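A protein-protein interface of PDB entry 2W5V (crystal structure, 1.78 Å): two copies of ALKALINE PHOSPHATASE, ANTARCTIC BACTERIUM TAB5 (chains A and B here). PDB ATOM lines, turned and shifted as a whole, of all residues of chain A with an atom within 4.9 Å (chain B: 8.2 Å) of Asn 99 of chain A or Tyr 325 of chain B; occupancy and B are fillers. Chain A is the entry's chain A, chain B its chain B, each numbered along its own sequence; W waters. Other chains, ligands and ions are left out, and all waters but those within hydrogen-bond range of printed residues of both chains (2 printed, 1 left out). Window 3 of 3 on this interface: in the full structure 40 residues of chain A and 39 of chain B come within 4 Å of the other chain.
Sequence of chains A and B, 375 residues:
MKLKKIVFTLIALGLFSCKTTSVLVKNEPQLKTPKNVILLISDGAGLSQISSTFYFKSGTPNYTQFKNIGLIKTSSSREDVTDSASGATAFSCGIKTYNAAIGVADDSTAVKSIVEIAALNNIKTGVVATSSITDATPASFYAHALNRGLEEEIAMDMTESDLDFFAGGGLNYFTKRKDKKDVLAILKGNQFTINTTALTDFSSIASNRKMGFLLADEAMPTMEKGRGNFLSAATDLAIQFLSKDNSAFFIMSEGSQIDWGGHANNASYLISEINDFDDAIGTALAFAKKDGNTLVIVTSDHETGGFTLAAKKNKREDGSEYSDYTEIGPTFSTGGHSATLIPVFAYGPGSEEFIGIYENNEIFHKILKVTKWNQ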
ATOM      1  N   SER A  76      29.955  -7.429  23.441  1.00  0.00           N
ATOM      2  CA  SER A  76      30.556  -6.217  23.991  1.00  0.00           C
ATOM      3  C   SER A  76      29.495  -5.426  24.758  1.00  0.00           C
ATOM      4  O   SER A  76      28.388  -5.917  24.981  1.00  0.00           O
ATOM      5  CB  SER A  76      31.162  -5.365  22.875  1.00  0.00           C
ATOM      6  OG  SER A  76      30.132  -4.738  22.122  1.00  0.00           O
ATOM      7  N   GLU A  79      27.405  -4.292  21.426  1.00  0.00           N
ATOM      8  CA  GLU A  79      27.237  -5.156  20.258  1.00  0.00           C
ATOM      9  C   GLU A  79      27.124  -6.637  20.638  1.00  0.00           C
ATOM     10  O   GLU A  79      27.930  -7.153  21.417  1.00  0.00           O
ATOM     11  CB  GLU A  79      28.411  -4.953  19.290  1.00  0.00           C
ATOM     12  CG  GLU A  79      28.471  -3.543  18.636  1.00  0.00           C
ATOM     13  CD  GLU A  79      29.514  -2.603  19.258  1.00  0.00           C
ATOM     14  OE1 GLU A  79      30.226  -3.004  20.203  1.00  0.00           O
ATOM     15  OE2 GLU A  79      29.631  -1.447  18.795  1.00  0.00           O
ATOM     16  N   ASP A  80      26.135  -7.324  20.069  1.00  0.00           N
ATOM     17  CA  ASP A  80      26.002  -8.768  20.269  1.00  0.00           C
ATOM     18  C   ASP A  80      27.226  -9.508  19.749  1.00  0.00           C
ATOM     19  O   ASP A  80      27.676 -10.485  20.355  1.00  0.00           O
ATOM     20  CB  ASP A  80      24.743  -9.307  19.578  1.00  0.00           C
ATOM     21  CG  ASP A  80      23.488  -9.144  20.425  1.00  0.00           C
ATOM     22  OD1 ASP A  80      23.602  -8.744  21.602  1.00  0.00           O
ATOM     23  OD2 ASP A  80      22.385  -9.433  19.916  1.00  0.00           O
ATOM     24  N   VAL A  81      27.747  -9.052  18.613  1.00  0.00           N
ATOM     25  CA  VAL A  81      28.947  -9.642  18.023  1.00  0.00           C
ATOM     26  C   VAL A  81      30.165  -8.767  18.315  1.00  0.00           C
ATOM     27  O   VAL A  81      30.243  -7.615  17.893  1.00  0.00           O
ATOM     28  CB  VAL A  81      28.793  -9.851  16.502  1.00  0.00           C
ATOM     29  CG1 VAL A  81      30.024 -10.547  15.920  1.00  0.00           C
ATOM     30  CG2 VAL A  81      27.520 -10.656  16.205  1.00  0.00           C
ATOM     31  N   THR A  82      31.124  -9.321  19.041  1.00  0.00           N
ATOM     32  CA  THR A  82      32.268  -8.533  19.466  1.00  0.00           C
ATOM     33  C   THR A  82      33.347  -8.427  18.385  1.00  0.00           C
ATOM     34  O   THR A  82      33.391  -9.236  17.457  1.00  0.00           O
ATOM     35  CB  THR A  82      32.869  -9.116  20.760  1.00  0.00           C
ATOM     36  OG1 THR A  82      33.843  -8.211  21.291  1.00  0.00           O
ATOM     37  CG2 THR A  82      33.512 -10.482  20.492  1.00  0.00           C
ATOM     38  N   ASP A  83      34.206  -7.413  18.489  1.00  0.00           N
ATOM     39  CA  ASP A  83      35.435  -7.412  17.704  1.00  0.00           C
ATOM     40  C   ASP A  83      36.598  -7.722  18.627  1.00  0.00           C
ATOM     41  O   ASP A  83      36.403  -7.937  19.831  1.00  0.00           O
ATOM     42  CB  ASP A  83      35.654  -6.097  16.924  1.00  0.00           C
ATOM     43  CG  ASP A  83      36.272  -4.987  17.776  1.00  0.00           C
ATOM     44  OD1 ASP A  83      36.023  -4.959  19.000  1.00  0.00           O
ATOM     45  OD2 ASP A  83      36.994  -4.130  17.211  1.00  0.00           O
ATOM     46  N   SER A  86      37.369  -4.953  21.810  1.00  0.00           N
ATOM     47  CA  SER A  86      36.542  -5.059  23.012  1.00  0.00           C
ATOM     48  C   SER A  86      36.691  -6.434  23.660  1.00  0.00           C
ATOM     49  O   SER A  86      36.716  -6.554  24.894  1.00  0.00           O
ATOM     50  CB  SER A  86      35.065  -4.789  22.708  1.00  0.00           C
ATOM     51  OG  SER A  86      34.610  -5.586  21.632  1.00  0.00           O
ATOM     52  N   THR A  97      33.239  -3.275  27.020  1.00  0.00           N
ATOM     53  CA  THR A  97      33.430  -1.968  26.378  1.00  0.00           C
ATOM     54  C   THR A  97      33.006  -2.045  24.914  1.00  0.00           C
ATOM     55  O   THR A  97      32.604  -3.111  24.450  1.00  0.00           O
ATOM     56  CB  THR A  97      34.881  -1.465  26.519  1.00  0.00           C
ATOM     57  OG1 THR A  97      34.965  -0.104  26.092  1.00  0.00           O
ATOM     58  CG2 THR A  97      35.843  -2.307  25.697  1.00  0.00           C
ATOM     59  N   TYR A  98      33.082  -0.924  24.198  1.00  0.00           N
ATOM     60  CA  TYR A  98      32.569  -0.871  22.831  1.00  0.00           C
ATOM     61  C   TYR A  98      33.552  -1.457  21.819  1.00  0.00           C
ATOM     62  O   TYR A  98      34.772  -1.368  22.010  1.00  0.00           O
ATOM     63  CB  TYR A  98      32.169   0.564  22.453  1.00  0.00           C
ATOM     64  CG  TYR A  98      33.275   1.602  22.586  1.00  0.00           C
ATOM     65  CD1 TYR A  98      34.201   1.793  21.567  1.00  0.00           C
ATOM     66  CD2 TYR A  98      33.381   2.395  23.720  1.00  0.00           C
ATOM     67  CE1 TYR A  98      35.217   2.741  21.682  1.00  0.00           C
ATOM     68  CE2 TYR A  98      34.395   3.348  23.843  1.00  0.00           C
ATOM     69  CZ  TYR A  98      35.310   3.510  22.817  1.00  0.00           C
ATOM     70  OH  TYR A  98      36.316   4.451  22.915  1.00  0.00           O
ATOM     71  N   ASN A  99      33.026  -2.069  20.756  1.00  0.00           N
ATOM     72  CA  ASN A  99      33.864  -2.593  19.674  1.00  0.00           C
ATOM     73  C   ASN A  99      34.826  -1.505  19.210  1.00  0.00           C
ATOM     74  O   ASN A  99      34.418  -0.352  19.027  1.00  0.00           O
ATOM     75  CB  ASN A  99      33.008  -3.076  18.489  1.00  0.00           C
ATOM     76  CG  ASN A  99      32.365  -4.440  18.735  1.00  0.00           C
ATOM     77  OD1 ASN A  99      32.593  -5.069  19.768  1.00  0.00           O
ATOM     78  ND2 ASN A  99      31.568  -4.906  17.777  1.00  0.00           N
ATOM     79  N   ALA A 100      36.095  -1.876  19.041  1.00  0.00           N
ATOM     80  CA  ALA A 100      37.183  -0.946  18.678  1.00  0.00           C
ATOM     81  C   ALA A 100      37.928  -0.306  19.862  1.00  0.00           C
ATOM     82  O   ALA A 100      39.026   0.225  19.691  1.00  0.00           O
ATOM     83  CB  ALA A 100      36.703   0.124  17.702  1.00  0.00           C
ATOM     84  N   ALA A 101      37.355  -0.356  21.058  1.00  0.00           N
ATOM     85  CA  ALA A 101      38.046   0.211  22.221  1.00  0.00           C
ATOM     86  C   ALA A 101      39.281  -0.594  22.628  1.00  0.00           C
ATOM     87  O   ALA A 101      39.283  -1.826  22.579  1.00  0.00           O
ATOM     88  CB  ALA A 101      37.099   0.354  23.402  1.00  0.00           C
ATOM     89  N   HIS A 263      38.296 -15.108   8.343  1.00  0.00           N
ATOM     90  CA  HIS A 263      37.773 -14.021   7.528  1.00  0.00           C
ATOM     91  C   HIS A 263      37.882 -14.345   6.054  1.00  0.00           C
ATOM     92  O   HIS A 263      36.996 -14.013   5.274  1.00  0.00           O
ATOM     93  CB  HIS A 263      38.513 -12.716   7.800  1.00  0.00           C
ATOM     94  CG  HIS A 263      38.075 -12.027   9.052  1.00  0.00           C
ATOM     95  ND1 HIS A 263      36.785 -11.577   9.241  1.00  0.00           N
ATOM     96  CD2 HIS A 263      38.755 -11.705  10.178  1.00  0.00           C
ATOM     97  CE1 HIS A 263      36.689 -11.007  10.428  1.00  0.00           C
ATOM     98  NE2 HIS A 263      37.875 -11.062  11.012  1.00  0.00           N
ATOM     99  N   GLY A 336      32.604 -12.712   8.659  1.00  0.00           N
ATOM    100  CA  GLY A 336      32.882 -11.966   9.878  1.00  0.00           C
ATOM    101  C   GLY A 336      32.869 -12.814  11.132  1.00  0.00           C
ATOM    102  O   GLY A 336      32.888 -14.056  11.057  1.00  0.00           O
ATOM    103  N   HIS A 337      32.830 -12.144  12.285  1.00  0.00           N
ATOM    104  CA  HIS A 337      32.791 -12.819  13.581  1.00  0.00           C
ATOM    105  C   HIS A 337      31.398 -13.357  13.882  1.00  0.00           C
ATOM    106  O   HIS A 337      30.421 -12.943  13.265  1.00  0.00           O
ATOM    107  CB  HIS A 337      33.192 -11.866  14.721  1.00  0.00           C
ATOM    108  CG  HIS A 337      34.545 -11.240  14.552  1.00  0.00           C
ATOM    109  ND1 HIS A 337      34.953 -10.149  15.285  1.00  0.00           N
ATOM    110  CD2 HIS A 337      35.572 -11.540  13.721  1.00  0.00           C
ATOM    111  CE1 HIS A 337      36.180  -9.808  14.925  1.00  0.00           C
ATOM    112  NE2 HIS A 337      36.575 -10.633  13.973  1.00  0.00           N
ATOM    113  N   LEU B 309      26.042 -17.883  14.801  1.00  0.00           N
ATOM    114  CA  LEU B 309      25.443 -16.639  15.292  1.00  0.00           C
ATOM    115  C   LEU B 309      26.155 -15.434  14.662  1.00  0.00           C
ATOM    116  O   LEU B 309      26.805 -14.636  15.347  1.00  0.00           O
ATOM    117  CB  LEU B 309      25.495 -16.576  16.826  1.00  0.00           C
ATOM    118  CG  LEU B 309      24.674 -17.670  17.519  1.00  0.00           C
ATOM    119  CD1 LEU B 309      24.847 -17.613  19.027  1.00  0.00           C
ATOM    120  CD2 LEU B 309      23.205 -17.539  17.143  1.00  0.00           C
ATOM    121  N   ALA B 310      26.022 -15.321  13.345  1.00  0.00           N
ATOM    122  CA  ALA B 310      26.697 -14.284  12.572  1.00  0.00           C
ATOM    123  C   ALA B 310      26.074 -12.921  12.809  1.00  0.00           C
ATOM    124  O   ALA B 310      24.945 -12.812  13.299  1.00  0.00           O
ATOM    125  CB  ALA B 310      26.654 -14.625  11.070  1.00  0.00           C
ATOM    126  N   ALA B 311      26.816 -11.882  12.445  1.00  0.00           N
ATOM    127  CA  ALA B 311      26.295 -10.529  12.473  1.00  0.00           C
ATOM    128  C   ALA B 311      25.126 -10.398  11.510  1.00  0.00           C
ATOM    129  O   ALA B 311      25.152 -10.936  10.401  1.00  0.00           O
ATOM    130  CB  ALA B 311      27.376  -9.550  12.093  1.00  0.00           C
ATOM    131  N   LYS B 312      24.104  -9.675  11.944  1.00  0.00           N
ATOM    132  CA  LYS B 312      22.968  -9.343  11.092  1.00  0.00           C
ATOM    133  C   LYS B 312      23.455  -8.630   9.840  1.00  0.00           C
ATOM    134  O   LYS B 312      24.414  -7.861   9.883  1.00  0.00           O
ATOM    135  CB  LYS B 312      22.017  -8.419  11.861  1.00  0.00           C
ATOM    136  CG  LYS B 312      20.668  -8.215  11.205  1.00  0.00           C
ATOM    137  CD  LYS B 312      19.747  -9.398  11.469  1.00  0.00           C
ATOM    138  CE  LYS B 312      18.432  -9.244  10.720  1.00  0.00           C
ATOM    139  NZ  LYS B 312      17.819  -7.903  10.945  1.00  0.00           N
ATOM    140  N   LYS B 313      22.797  -8.882   8.719  1.00  0.00           N
ATOM    141  CA  LYS B 313      23.154  -8.200   7.488  1.00  0.00           C
ATOM    142  C   LYS B 313      22.222  -7.023   7.241  1.00  0.00           C
ATOM    143  O   LYS B 313      21.004  -7.175   7.246  1.00  0.00           O
ATOM    144  CB  LYS B 313      23.129  -9.169   6.308  1.00  0.00           C
ATOM    145  CG  LYS B 313      24.467  -9.826   6.036  1.00  0.00           C
ATOM    146  CD  LYS B 313      24.302 -11.263   5.563  1.00  0.00           C
ATOM    147  CE  LYS B 313      25.504 -11.707   4.745  1.00  0.00           C
ATOM    148  NZ  LYS B 313      26.752 -11.001   5.152  1.00  0.00           N
ATOM    149  N   ASN B 314      22.804  -5.844   7.050  1.00  0.00           N
ATOM    150  CA  ASN B 314      22.034  -4.674   6.659  1.00  0.00           C
ATOM    151  C   ASN B 314      22.190  -4.413   5.171  1.00  0.00           C
ATOM    152  O   ASN B 314      23.195  -4.792   4.566  1.00  0.00           O
ATOM    153  CB  ASN B 314      22.459  -3.446   7.458  1.00  0.00           C
ATOM    154  CG  ASN B 314      21.912  -3.455   8.868  1.00  0.00           C
ATOM    155  OD1 ASN B 314      21.116  -4.323   9.232  1.00  0.00           O
ATOM    156  ND2 ASN B 314      22.334  -2.485   9.673  1.00  0.00           N
ATOM    157  N   TYR B 322      26.103  -5.262   4.036  1.00  0.00           N
ATOM    158  CA  TYR B 322      27.200  -5.056   4.976  1.00  0.00           C
ATOM    159  C   TYR B 322      26.816  -5.601   6.352  1.00  0.00           C
ATOM    160  O   TYR B 322      25.637  -5.676   6.698  1.00  0.00           O
ATOM    161  CB  TYR B 322      27.570  -3.573   5.077  1.00  0.00           C
ATOM    162  CG  TYR B 322      26.567  -2.731   5.833  1.00  0.00           C
ATOM    163  CD1 TYR B 322      26.654  -2.583   7.213  1.00  0.00           C
ATOM    164  CD2 TYR B 322      25.540  -2.072   5.168  1.00  0.00           C
ATOM    165  CE1 TYR B 322      25.741  -1.814   7.911  1.00  0.00           C
ATOM    166  CE2 TYR B 322      24.622  -1.298   5.858  1.00  0.00           C
ATOM    167  CZ  TYR B 322      24.729  -1.174   7.230  1.00  0.00           C
ATOM    168  OH  TYR B 322      23.820  -0.408   7.923  1.00  0.00           O
ATOM    169  N   SER B 323      27.816  -5.976   7.138  1.00  0.00           N
ATOM    170  CA  SER B 323      27.563  -6.631   8.416  1.00  0.00           C
ATOM    171  C   SER B 323      27.320  -5.628   9.535  1.00  0.00           C
ATOM    172  O   SER B 323      28.048  -4.647   9.679  1.00  0.00           O
ATOM    173  CB  SER B 323      28.731  -7.545   8.782  1.00  0.00           C
ATOM    174  OG  SER B 323      29.016  -8.438   7.726  1.00  0.00           O
ATOM    175  N   ASP B 324      26.289  -5.880  10.329  1.00  0.00           N
ATOM    176  CA  ASP B 324      25.996  -5.029  11.472  1.00  0.00           C
ATOM    177  C   ASP B 324      26.176  -5.844  12.751  1.00  0.00           C
ATOM    178  O   ASP B 324      25.346  -6.689  13.084  1.00  0.00           O
ATOM    179  CB  ASP B 324      24.575  -4.482  11.376  1.00  0.00           C
ATOM    180  CG  ASP B 324      24.181  -3.678  12.593  1.00  0.00           C
ATOM    181  OD1 ASP B 324      25.053  -3.444  13.458  1.00  0.00           O
ATOM    182  OD2 ASP B 324      22.999  -3.286  12.684  1.00  0.00           O
ATOM    183  N   TYR B 325      27.269  -5.582  13.457  1.00  0.00           N
ATOM    184  CA  TYR B 325      27.655  -6.388  14.611  1.00  0.00           C
ATOM    185  C   TYR B 325      26.758  -6.156  15.821  1.00  0.00           C
ATOM    186  O   TYR B 325      26.855  -6.882  16.812  1.00  0.00           O
ATOM    187  CB  TYR B 325      29.119  -6.127  14.987  1.00  0.00           C
ATOM    188  CG  TYR B 325      30.137  -6.936  14.200  1.00  0.00           C
ATOM    189  CD1 TYR B 325      29.870  -7.358  12.906  1.00  0.00           C
ATOM    190  CD2 TYR B 325      31.379  -7.249  14.745  1.00  0.00           C
ATOM    191  CE1 TYR B 325      30.797  -8.095  12.182  1.00  0.00           C
ATOM    192  CE2 TYR B 325      32.321  -7.979  14.021  1.00  0.00           C
ATOM    193  CZ  TYR B 325      32.021  -8.394  12.744  1.00  0.00           C
ATOM    194  OH  TYR B 325      32.945  -9.119  12.026  1.00  0.00           O
ATOM    195  N   THR B 326      25.877  -5.160  15.752  1.00  0.00           N
ATOM    196  CA  THR B 326      25.002  -4.897  16.894  1.00  0.00           C
ATOM    197  C   THR B 326      24.056  -6.057  17.161  1.00  0.00           C
ATOM    198  O   THR B 326      23.769  -6.360  18.312  1.00  0.00           O
ATOM    199  CB  THR B 326      24.168  -3.615  16.733  1.00  0.00           C
ATOM    200  OG1 THR B 326      23.456  -3.665  15.490  1.00  0.00           O
ATOM    201  CG2 THR B 326      25.072  -2.398  16.760  1.00  0.00           C
ATOM    202  N   GLU B 327      23.585  -6.708  16.097  1.00  0.00           N
ATOM    203  CA  GLU B 327      22.618  -7.798  16.219  1.00  0.00           C
ATOM    204  C   GLU B 327      23.064  -9.055  15.486  1.00  0.00           C
ATOM    205  O   GLU B 327      23.984  -9.026  14.670  1.00  0.00           O
ATOM    206  CB  GLU B 327      21.261  -7.408  15.631  1.00  0.00           C
ATOM    207  CG  GLU B 327      20.616  -6.170  16.220  1.00  0.00           C
ATOM    208  CD  GLU B 327      19.243  -5.930  15.628  1.00  0.00           C
ATOM    209  OE1 GLU B 327      18.951  -4.782  15.230  1.00  0.00           O
ATOM    210  OE2 GLU B 327      18.462  -6.903  15.541  1.00  0.00           O
ATOM    211  N   ILE B 328      22.357 -10.145  15.759  1.00  0.00           N
ATOM    212  CA  ILE B 328      22.682 -11.453  15.208  1.00  0.00           C
ATOM    213  C   ILE B 328      21.717 -11.875  14.103  1.00  0.00           C
ATOM    214  O   ILE B 328      20.500 -11.739  14.244  1.00  0.00           O
ATOM    215  CB  ILE B 328      22.655 -12.523  16.315  1.00  0.00           C
ATOM    216  CG1 ILE B 328      23.814 -12.311  17.287  1.00  0.00           C
ATOM    217  CG2 ILE B 328      22.710 -13.918  15.708  1.00  0.00           C
ATOM    218  CD1 ILE B 328      23.666 -13.086  18.597  1.00  0.00           C
ATOM    219  N   GLY B 329      22.270 -12.387  13.005  1.00  0.00           N
ATOM    220  CA  GLY B 329      21.486 -13.032  11.963  1.00  0.00           C
ATOM    221  C   GLY B 329      22.019 -14.439  11.720  1.00  0.00           C
ATOM    222  O   GLY B 329      23.039 -14.611  11.052  1.00  0.00           O
HETATM  223  O   HOH W   1      29.411 -12.226  10.856  1.00  0.00           O
HETATM  224  O   HOH W   2      20.496 -10.365  18.606  1.00  0.00           O
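Water W2 bridges the side-chain carboxylate (OD2) of Asp 80 of chain A (2.5 Å) and the backbone NH (N) of Ile 328 of chain B (3.4 Å).
Water W1 lies within hydrogen-bond range of O of His 337 of chain A and N of Ala 311 of chain B.
Asn 99 of chain A touches just one residue of chain B: Tyr 325.
Of chain A, only Glu 79, Asp 80, Val 81, Thr 82, Asn 99, Gly 336 and His 337 come within 4 Å of Tyr 325 of chain B.
Of the printed residues of chain B, Asp 80 of chain A touches Tyr 325 (3.4 Å), Thr 326 (3.1 Å) and Ile 328 (3.9 Å).
Printed residues of chain B within 4 Å of His 337 of chain A: Ala 311 (3.8 Å) and Tyr 325 (3.0 Å).
Of the printed residues of chain A, Ile 328 of chain B touches Asp 80.
The nearest residue of chain A that does not touch Tyr 325 of chain B is His 263 of chain A (4.5 Å).
The backbone NH (N) of Asp 80 of chain A is in hydrogen-bond range of the backbone carbonyl oxygen (O) of Thr 326 of chain B.
The backbone NH (N) of His 337 of chain A lies within hydrogen-bond range of the side-chain hydroxyl (OH) of Tyr 325 of chain B (3.0 Å).
The backbone NH (N) of Val 81 of chain A is in hydrogen-bond range of the backbone carbonyl oxygen (O) of Tyr 325 of chain B (3.0 Å).
The backbone NH of Asp 80 of chain A is in hydrogen-bond range of the backbone carbonyl oxygen of Tyr 325 of chain B (3.4 Å).
The side-chain hydroxyl (OG1) of Thr 326 of chain B is in hydrogen-bond range of the side-chain carboxylate (OD1) of Asp 324 of chain B (2.6 Å).
The backbone carbonyl oxygen of Val 81 of chain A lies within hydrogen-bond range of the side-chain amide nitrogen of Asn 99 of chain A (3.0 Å).
OG of Ser 76 of chain A lies within hydrogen-bond range of OE1 of Glu 79 of chain A (2.6 Å).
The backbone NH (N) of Asp 83 of chain A sits at hydrogen-bond distance from the side-chain amide oxygen (OD1) of Asn 99 of chain A (3.1 Å).
The side-chain hydroxyl (OG) of Ser 86 of chain A sits at hydrogen-bond distance from the side-chain amide oxygen (OD1) of Asn 99 of chain A (2.8 Å).
The side-chain hydroxyl of Ser 76 of chain A lies within hydrogen-bond range of the side-chain amide oxygen of Asn 99 of chain A (3.4 Å).
Among the printed residues, pairs that only touch across the chains: Glu 79 of chain A with Tyr 325 of chain B, Gly 336 of chain A with Tyr 325 of chain B, Thr 82 of chain A with Tyr 325 of chain B, Asn 99 of chain A with Tyr 325 of chain B, His 337 of chain A with Ala 311 of chain B, Asp 80 of chain A with Ile 328 of chain B and Val 81 of chain A with Ala 311 of chain B.
Along chain A the printed residues that touch a printed residue of chain B span positions 79 to 337.
Hydrophobic or aromatic side chains of chain B that line the printed part of chain A: Tyr 325 and Ile 328.
No position is printed for both chains.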
